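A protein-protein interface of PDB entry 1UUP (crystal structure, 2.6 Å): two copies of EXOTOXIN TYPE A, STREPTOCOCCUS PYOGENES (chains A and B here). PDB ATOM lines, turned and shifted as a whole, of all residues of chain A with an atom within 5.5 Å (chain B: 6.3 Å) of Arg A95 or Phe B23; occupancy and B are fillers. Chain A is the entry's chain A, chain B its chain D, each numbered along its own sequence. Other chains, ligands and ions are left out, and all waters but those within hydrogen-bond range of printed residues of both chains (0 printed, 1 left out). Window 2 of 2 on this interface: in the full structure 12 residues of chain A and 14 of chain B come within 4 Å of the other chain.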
ATOM      1  N   GLY A  52      21.566 -13.757 -14.129  1.00  0.00           N
ATOM      2  CA  GLY A  52      20.612 -14.106 -15.152  1.00  0.00           C
ATOM      3  C   GLY A  52      19.532 -13.059 -15.014  1.00  0.00           C
ATOM      4  O   GLY A  52      19.758 -12.050 -14.351  1.00  0.00           O
ATOM      5  N   ASN A  54      16.593 -11.124 -13.384  1.00  0.00           N
ATOM      6  CA  ASN A  54      16.159 -11.140 -11.979  1.00  0.00           C
ATOM      7  C   ASN A  54      17.213 -11.337 -10.881  1.00  0.00           C
ATOM      8  O   ASN A  54      16.966 -10.964  -9.734  1.00  0.00           O
ATOM      9  CB  ASN A  54      15.088 -12.220 -11.763  1.00  0.00           C
ATOM     10  CG  ASN A  54      13.920 -12.099 -12.719  1.00  0.00           C
ATOM     11  OD1 ASN A  54      12.996 -12.913 -12.687  1.00  0.00           O
ATOM     12  ND2 ASN A  54      13.952 -11.084 -13.576  1.00  0.00           N
ATOM     13  N   TYR A  55      18.361 -11.928 -11.193  1.00  0.00           N
ATOM     14  CA  TYR A  55      19.372 -12.152 -10.153  1.00  0.00           C
ATOM     15  C   TYR A  55      20.816 -12.000 -10.628  1.00  0.00           C
ATOM     16  O   TYR A  55      21.116 -12.182 -11.806  1.00  0.00           O
ATOM     17  CB  TYR A  55      19.199 -13.559  -9.561  1.00  0.00           C
ATOM     18  CG  TYR A  55      19.750 -14.662 -10.448  1.00  0.00           C
ATOM     19  CD1 TYR A  55      21.100 -15.027 -10.395  1.00  0.00           C
ATOM     20  CD2 TYR A  55      18.926 -15.325 -11.353  1.00  0.00           C
ATOM     21  CE1 TYR A  55      21.612 -16.030 -11.223  1.00  0.00           C
ATOM     22  CE2 TYR A  55      19.424 -16.329 -12.184  1.00  0.00           C
ATOM     23  CZ  TYR A  55      20.763 -16.680 -12.115  1.00  0.00           C
ATOM     24  OH  TYR A  55      21.235 -17.684 -12.929  1.00  0.00           O
ATOM     25  N   ASP A  56      21.712 -11.688  -9.695  1.00  0.00           N
ATOM     26  CA  ASP A  56      23.130 -11.544 -10.023  1.00  0.00           C
ATOM     27  C   ASP A  56      23.998 -12.253  -8.989  1.00  0.00           C
ATOM     28  O   ASP A  56      25.220 -12.101  -8.974  1.00  0.00           O
ATOM     29  CB  ASP A  56      23.524 -10.074 -10.090  1.00  0.00           C
ATOM     30  CG  ASP A  56      23.143  -9.338  -8.849  1.00  0.00           C
ATOM     31  OD1 ASP A  56      22.310  -8.410  -8.948  1.00  0.00           O
ATOM     32  OD2 ASP A  56      23.667  -9.702  -7.773  1.00  0.00           O
ATOM     33  N   LYS A  57      23.354 -13.031  -8.130  1.00  0.00           N
ATOM     34  CA  LYS A  57      24.048 -13.780  -7.097  1.00  0.00           C
ATOM     35  C   LYS A  57      23.218 -15.051  -6.859  1.00  0.00           C
ATOM     36  O   LYS A  57      21.998 -14.995  -6.682  1.00  0.00           O
ATOM     37  CB  LYS A  57      24.167 -12.919  -5.837  1.00  0.00           C
ATOM     38  CG  LYS A  57      25.488 -13.079  -5.096  1.00  0.00           C
ATOM     39  CD  LYS A  57      25.750 -11.901  -4.136  1.00  0.00           C
ATOM     40  CE  LYS A  57      26.734 -10.877  -4.736  1.00  0.00           C
ATOM     41  NZ  LYS A  57      26.347 -10.396  -6.107  1.00  0.00           N
ATOM     42  N   ALA A  93      22.203  -8.136  -0.006  1.00  0.00           N
ATOM     43  CA  ALA A  93      22.104  -8.870  -1.258  1.00  0.00           C
ATOM     44  C   ALA A  93      20.597  -8.880  -1.475  1.00  0.00           C
ATOM     45  O   ALA A  93      19.859  -9.534  -0.737  1.00  0.00           O
ATOM     46  CB  ALA A  93      22.635 -10.282  -1.103  1.00  0.00           C
ATOM     47  N   GLU A  94      20.143  -8.120  -2.462  1.00  0.00           N
ATOM     48  CA  GLU A  94      18.722  -8.020  -2.740  1.00  0.00           C
ATOM     49  C   GLU A  94      18.325  -8.634  -4.063  1.00  0.00           C
ATOM     50  O   GLU A  94      17.182  -8.490  -4.484  1.00  0.00           O
ATOM     51  CB  GLU A  94      18.293  -6.560  -2.741  1.00  0.00           C
ATOM     52  CG  GLU A  94      18.930  -5.726  -1.663  1.00  0.00           C
ATOM     53  CD  GLU A  94      18.138  -4.470  -1.388  1.00  0.00           C
ATOM     54  OE1 GLU A  94      18.731  -3.486  -0.901  1.00  0.00           O
ATOM     55  OE2 GLU A  94      16.917  -4.471  -1.652  1.00  0.00           O
ATOM     56  N   ARG A  95      19.256  -9.294  -4.739  1.00  0.00           N
ATOM     57  CA  ARG A  95      18.930  -9.913  -6.011  1.00  0.00           C
ATOM     58  C   ARG A  95      19.530 -11.313  -6.129  1.00  0.00           C
ATOM     59  O   ARG A  95      20.195 -11.660  -7.112  1.00  0.00           O
ATOM     60  CB  ARG A  95      19.372  -8.995  -7.151  1.00  0.00           C
ATOM     61  CG  ARG A  95      18.357  -7.874  -7.410  1.00  0.00           C
ATOM     62  CD  ARG A  95      18.841  -6.828  -8.392  1.00  0.00           C
ATOM     63  NE  ARG A  95      19.634  -7.375  -9.493  1.00  0.00           N
ATOM     64  CZ  ARG A  95      19.153  -7.786 -10.659  1.00  0.00           C
ATOM     65  NH1 ARG A  95      17.856  -7.725 -10.910  1.00  0.00           N
ATOM     66  NH2 ARG A  95      19.988  -8.237 -11.584  1.00  0.00           N
ATOM     67  N   SER A  96      19.267 -12.124  -5.112  1.00  0.00           N
ATOM     68  CA  SER A  96      19.785 -13.478  -5.078  1.00  0.00           C
ATOM     69  C   SER A  96      18.750 -14.482  -5.547  1.00  0.00           C
ATOM     70  O   SER A  96      17.553 -14.228  -5.495  1.00  0.00           O
ATOM     71  CB  SER A  96      20.233 -13.834  -3.653  1.00  0.00           C
ATOM     72  OG  SER A  96      21.141 -12.867  -3.138  1.00  0.00           O
ATOM     73  N   ALA A  97      19.226 -15.622  -6.022  1.00  0.00           N
ATOM     74  CA  ALA A  97      18.348 -16.692  -6.472  1.00  0.00           C
ATOM     75  C   ALA A  97      18.772 -17.866  -5.623  1.00  0.00           C
ATOM     76  O   ALA A  97      19.896 -17.895  -5.124  1.00  0.00           O
ATOM     77  CB  ALA A  97      18.573 -16.991  -7.947  1.00  0.00           C
ATOM     78  N   LEU B  18      24.916   0.167  -5.980  1.00  0.00           N
ATOM     79  CA  LEU B  18      24.011   1.120  -6.605  1.00  0.00           C
ATOM     80  C   LEU B  18      23.314   0.496  -7.806  1.00  0.00           C
ATOM     81  O   LEU B  18      22.474   1.125  -8.441  1.00  0.00           O
ATOM     82  CB  LEU B  18      24.791   2.368  -7.048  1.00  0.00           C
ATOM     83  CG  LEU B  18      24.082   3.485  -7.821  1.00  0.00           C
ATOM     84  CD1 LEU B  18      23.046   4.177  -6.963  1.00  0.00           C
ATOM     85  CD2 LEU B  18      25.129   4.480  -8.296  1.00  0.00           C
ATOM     86  N   GLN B  19      23.654  -0.748  -8.122  1.00  0.00           N
ATOM     87  CA  GLN B  19      23.035  -1.407  -9.269  1.00  0.00           C
ATOM     88  C   GLN B  19      21.601  -1.777  -8.942  1.00  0.00           C
ATOM     89  O   GLN B  19      20.769  -1.909  -9.838  1.00  0.00           O
ATOM     90  CB  GLN B  19      23.833  -2.646  -9.699  1.00  0.00           C
ATOM     91  CG  GLN B  19      23.855  -3.792  -8.694  1.00  0.00           C
ATOM     92  CD  GLN B  19      24.893  -3.628  -7.611  1.00  0.00           C
ATOM     93  OE1 GLN B  19      25.052  -4.504  -6.763  1.00  0.00           O
ATOM     94  NE2 GLN B  19      25.609  -2.509  -7.628  1.00  0.00           N
ATOM     95  N   ASN B  20      21.304  -1.922  -7.653  1.00  0.00           N
ATOM     96  CA  ASN B  20      19.942  -2.243  -7.231  1.00  0.00           C
ATOM     97  C   ASN B  20      18.989  -1.102  -7.617  1.00  0.00           C
ATOM     98  O   ASN B  20      17.855  -1.350  -8.040  1.00  0.00           O
ATOM     99  CB  ASN B  20      19.879  -2.499  -5.718  1.00  0.00           C
ATOM    100  CG  ASN B  20      20.668  -3.728  -5.304  1.00  0.00           C
ATOM    101  OD1 ASN B  20      20.640  -4.756  -5.981  1.00  0.00           O
ATOM    102  ND2 ASN B  20      21.369  -3.632  -4.183  1.00  0.00           N
ATOM    103  N   ILE B  21      19.440   0.143  -7.470  1.00  0.00           N
ATOM    104  CA  ILE B  21      18.606   1.267  -7.859  1.00  0.00           C
ATOM    105  C   ILE B  21      18.456   1.187  -9.381  1.00  0.00           C
ATOM    106  O   ILE B  21      17.379   1.436  -9.920  1.00  0.00           O
ATOM    107  CB  ILE B  21      19.243   2.630  -7.467  1.00  0.00           C
ATOM    108  CG1 ILE B  21      19.320   2.760  -5.938  1.00  0.00           C
ATOM    109  CG2 ILE B  21      18.421   3.783  -8.061  1.00  0.00           C
ATOM    110  CD1 ILE B  21      17.971   2.701  -5.229  1.00  0.00           C
ATOM    111  N   TYR B  22      19.541   0.826 -10.061  1.00  0.00           N
ATOM    112  CA  TYR B  22      19.542   0.683 -11.516  1.00  0.00           C
ATOM    113  C   TYR B  22      18.466  -0.300 -12.022  1.00  0.00           C
ATOM    114  O   TYR B  22      17.686   0.030 -12.921  1.00  0.00           O
ATOM    115  CB  TYR B  22      20.929   0.207 -11.996  1.00  0.00           C
ATOM    116  CG  TYR B  22      20.960  -0.306 -13.425  1.00  0.00           C
ATOM    117  CD1 TYR B  22      20.989   0.578 -14.510  1.00  0.00           C
ATOM    118  CD2 TYR B  22      20.916  -1.678 -13.696  1.00  0.00           C
ATOM    119  CE1 TYR B  22      20.967   0.114 -15.829  1.00  0.00           C
ATOM    120  CE2 TYR B  22      20.896  -2.155 -15.007  1.00  0.00           C
ATOM    121  CZ  TYR B  22      20.921  -1.254 -16.073  1.00  0.00           C
ATOM    122  OH  TYR B  22      20.892  -1.721 -17.379  1.00  0.00           O
ATOM    123  N   PHE B  23      18.426  -1.502 -11.452  1.00  0.00           N
ATOM    124  CA  PHE B  23      17.446  -2.511 -11.888  1.00  0.00           C
ATOM    125  C   PHE B  23      15.985  -2.123 -11.669  1.00  0.00           C
ATOM    126  O   PHE B  23      15.095  -2.653 -12.340  1.00  0.00           O
ATOM    127  CB  PHE B  23      17.709  -3.862 -11.215  1.00  0.00           C
ATOM    128  CG  PHE B  23      18.918  -4.554 -11.727  1.00  0.00           C
ATOM    129  CD1 PHE B  23      20.099  -4.553 -10.995  1.00  0.00           C
ATOM    130  CD2 PHE B  23      18.897  -5.180 -12.975  1.00  0.00           C
ATOM    131  CE1 PHE B  23      21.252  -5.158 -11.495  1.00  0.00           C
ATOM    132  CE2 PHE B  23      20.048  -5.795 -13.494  1.00  0.00           C
ATOM    133  CZ  PHE B  23      21.226  -5.783 -12.753  1.00  0.00           C
ATOM    134  N   LEU B  24      15.748  -1.210 -10.727  1.00  0.00           N
ATOM    135  CA  LEU B  24      14.395  -0.740 -10.432  1.00  0.00           C
ATOM    136  C   LEU B  24      13.887   0.192 -11.526  1.00  0.00           C
ATOM    137  O   LEU B  24      12.713   0.153 -11.888  1.00  0.00           O
ATOM    138  CB  LEU B  24      14.358   0.024  -9.107  1.00  0.00           C
ATOM    139  CG  LEU B  24      14.472  -0.688  -7.758  1.00  0.00           C
ATOM    140  CD1 LEU B  24      14.557   0.374  -6.657  1.00  0.00           C
ATOM    141  CD2 LEU B  24      13.276  -1.611  -7.542  1.00  0.00           C
ATOM    142  N   TYR B  25      14.759   1.040 -12.050  1.00  0.00           N
ATOM    143  CA  TYR B  25      14.316   1.968 -13.075  1.00  0.00           C
ATOM    144  C   TYR B  25      14.617   1.515 -14.499  1.00  0.00           C
ATOM    145  O   TYR B  25      14.116   2.096 -15.457  1.00  0.00           O
ATOM    146  CB  TYR B  25      14.896   3.368 -12.812  1.00  0.00           C
ATOM    147  CG  TYR B  25      14.390   3.990 -11.522  1.00  0.00           C
ATOM    148  CD1 TYR B  25      15.039   3.763 -10.310  1.00  0.00           C
ATOM    149  CD2 TYR B  25      13.228   4.759 -11.505  1.00  0.00           C
ATOM    150  CE1 TYR B  25      14.540   4.284  -9.112  1.00  0.00           C
ATOM    151  CE2 TYR B  25      12.716   5.286 -10.312  1.00  0.00           C
ATOM    152  CZ  TYR B  25      13.375   5.043  -9.118  1.00  0.00           C
ATOM    153  OH  TYR B  25      12.862   5.537  -7.933  1.00  0.00           O
ATOM    154  N   GLU B  26      15.426   0.477 -14.647  1.00  0.00           N
ATOM    155  CA  GLU B  26      15.737  -0.012 -15.983  1.00  0.00           C
ATOM    156  C   GLU B  26      14.650  -0.972 -16.457  1.00  0.00           C
ATOM    157  O   GLU B  26      14.295  -0.987 -17.636  1.00  0.00           O
ATOM    158  CB  GLU B  26      17.102  -0.711 -16.015  1.00  0.00           C
ATOM    159  CG  GLU B  26      17.363  -1.484 -17.314  1.00  0.00           C
ATOM    160  CD  GLU B  26      17.109  -0.642 -18.562  1.00  0.00           C
ATOM    161  OE1 GLU B  26      17.306  -1.156 -19.683  1.00  0.00           O
ATOM    162  OE2 GLU B  26      16.706   0.536 -18.427  1.00  0.00           O
ATOM    163  N   GLY B  27      14.123  -1.763 -15.526  1.00  0.00           N
ATOM    164  CA  GLY B  27      13.081  -2.719 -15.865  1.00  0.00           C
ATOM    165  C   GLY B  27      11.706  -2.094 -16.018  1.00  0.00           C
ATOM    166  O   GLY B  27      11.486  -0.931 -15.653  1.00  0.00           O
ATOM    167  N   ASP B  28      10.770  -2.862 -16.561  1.00  0.00           N
ATOM    168  CA  ASP B  28       9.417  -2.352 -16.744  1.00  0.00           C
ATOM    169  C   ASP B  28       8.741  -2.070 -15.416  1.00  0.00           C
ATOM    170  O   ASP B  28       9.054  -2.683 -14.394  1.00  0.00           O
ATOM    171  CB  ASP B  28       8.544  -3.338 -17.532  1.00  0.00           C
ATOM    172  CG  ASP B  28       8.960  -3.458 -18.978  1.00  0.00           C
ATOM    173  OD1 ASP B  28       9.380  -2.435 -19.567  1.00  0.00           O
ATOM    174  OD2 ASP B  28       8.855  -4.570 -19.531  1.00  0.00           O
ATOM    175  N   HIS B  85      12.857  -8.068  -2.823  1.00  0.00           N
ATOM    176  CA  HIS B  85      13.611  -8.370  -1.610  1.00  0.00           C
ATOM    177  C   HIS B  85      12.885  -7.854  -0.369  1.00  0.00           C
ATOM    178  O   HIS B  85      12.735  -6.649  -0.186  1.00  0.00           O
ATOM    179  CB  HIS B  85      15.015  -7.756  -1.679  1.00  0.00           C
ATOM    180  CG  HIS B  85      15.886  -8.113  -0.514  1.00  0.00           C
ATOM    181  ND1 HIS B  85      16.066  -9.414  -0.091  1.00  0.00           N
ATOM    182  CD2 HIS B  85      16.646  -7.346   0.304  1.00  0.00           C
ATOM    183  CE1 HIS B  85      16.900  -9.431   0.933  1.00  0.00           C
ATOM    184  NE2 HIS B  85      17.268  -8.190   1.193  1.00  0.00           N
ATOM    185  N   TYR B 160      21.910   5.585 -14.578  1.00  0.00           N
ATOM    186  CA  TYR B 160      22.147   4.388 -13.787  1.00  0.00           C
ATOM    187  C   TYR B 160      22.745   3.336 -14.713  1.00  0.00           C
ATOM    188  O   TYR B 160      22.540   3.389 -15.922  1.00  0.00           O
ATOM    189  CB  TYR B 160      20.828   3.858 -13.222  1.00  0.00           C
ATOM    190  CG  TYR B 160      20.141   4.772 -12.233  1.00  0.00           C
ATOM    191  CD1 TYR B 160      18.804   5.134 -12.397  1.00  0.00           C
ATOM    192  CD2 TYR B 160      20.812   5.236 -11.104  1.00  0.00           C
ATOM    193  CE1 TYR B 160      18.153   5.930 -11.456  1.00  0.00           C
ATOM    194  CE2 TYR B 160      20.174   6.032 -10.156  1.00  0.00           C
ATOM    195  CZ  TYR B 160      18.845   6.376 -10.332  1.00  0.00           C
ATOM    196  OH  TYR B 160      18.215   7.145  -9.367  1.00  0.00           O
ATOM    197  N   THR B 161      23.504   2.404 -14.151  1.00  0.00           N
ATOM    198  CA  THR B 161      24.081   1.301 -14.921  1.00  0.00           C
ATOM    199  C   THR B 161      24.210   0.154 -13.936  1.00  0.00           C
ATOM    200  O   THR B 161      24.044   0.348 -12.731  1.00  0.00           O
ATOM    201  CB  THR B 161      25.510   1.589 -15.475  1.00  0.00           C
ATOM    202  OG1 THR B 161      26.448   1.636 -14.396  1.00  0.00           O
ATOM    203  CG2 THR B 161      25.544   2.875 -16.257  1.00  0.00           C
ATOM    204  N   ASN B 162      24.484  -1.044 -14.430  1.00  0.00           N
ATOM    205  CA  ASN B 162      24.673  -2.154 -13.517  1.00  0.00           C
ATOM    206  C   ASN B 162      26.066  -1.881 -12.957  1.00  0.00           C
ATOM    207  O   ASN B 162      27.055  -2.515 -13.329  1.00  0.00           O
ATOM    208  CB  ASN B 162      24.619  -3.487 -14.261  1.00  0.00           C
ATOM    209  CG  ASN B 162      24.801  -4.672 -13.339  1.00  0.00           C
ATOM    210  OD1 ASN B 162      24.354  -4.653 -12.192  1.00  0.00           O
ATOM    211  ND2 ASN B 162      25.447  -5.717 -13.837  1.00  0.00           N
ATOM    212  N   GLN B 194      16.272  -1.460  -1.200  1.00  0.00           N
ATOM    213  CA  GLN B 194      15.286  -1.030  -2.188  1.00  0.00           C
ATOM    214  C   GLN B 194      13.991  -0.608  -1.518  1.00  0.00           C
ATOM    215  O   GLN B 194      13.389   0.409  -1.879  1.00  0.00           O
ATOM    216  CB  GLN B 194      14.979  -2.145  -3.194  1.00  0.00           C
ATOM    217  CG  GLN B 194      16.077  -2.437  -4.196  1.00  0.00           C
ATOM    218  CD  GLN B 194      15.747  -3.639  -5.068  1.00  0.00           C
ATOM    219  OE1 GLN B 194      15.407  -4.710  -4.557  1.00  0.00           O
ATOM    220  NE2 GLN B 194      15.849  -3.472  -6.386  1.00  0.00           N
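The backbone carbonyl oxygen (O) of Ala A93 lies close to a ring nitrogen (NE2) of His B85 (3.5 Å).
The backbone NH of Gln B194 is in hydrogen-bond range of the side-chain carboxylate of Glu A94 (3.1 Å).
OD1 of Asp A56 is in salt-bridge range of NE of Arg A95, 2.9 Å away.
NE2 of Gln B194 is in hydrogen-bond range of O of Asn B20, 3.4 Å away.
Among the printed residues, merely in contact across the chains: Glu A94 with His B85 (3.4 Å), Arg A95 with Asn B20 (3.7 Å) and Arg A95 with Phe B23 (3.0 Å).
Of the printed residues of chain B, Ala A93 touches His B85 (3.4 Å).
Of the printed residues of chain B, Glu A94 touches His B85 (3.4 Å) and Gln B194 (3.1 Å).
Arg A95 touches just these residues of chain B: Asn B20 and Phe B23.
Phe B23 touches one residue of chain A.
Of the printed residues of chain A, His B85 touches Ala A93 (3.4 Å) and Glu A94 (3.4 Å).
Printed residues of chain A within 4 Å of Gln B194: Glu A94 (3.1 Å).
Of the 16 printed residues of chain B, 4 touch a printed residue of chain A.
Among the printed residues, no Asp or Glu carboxylate lies within 4 Å of a Lys or Arg side-chain nitrogen of the other chain.
No position is printed for both chains.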
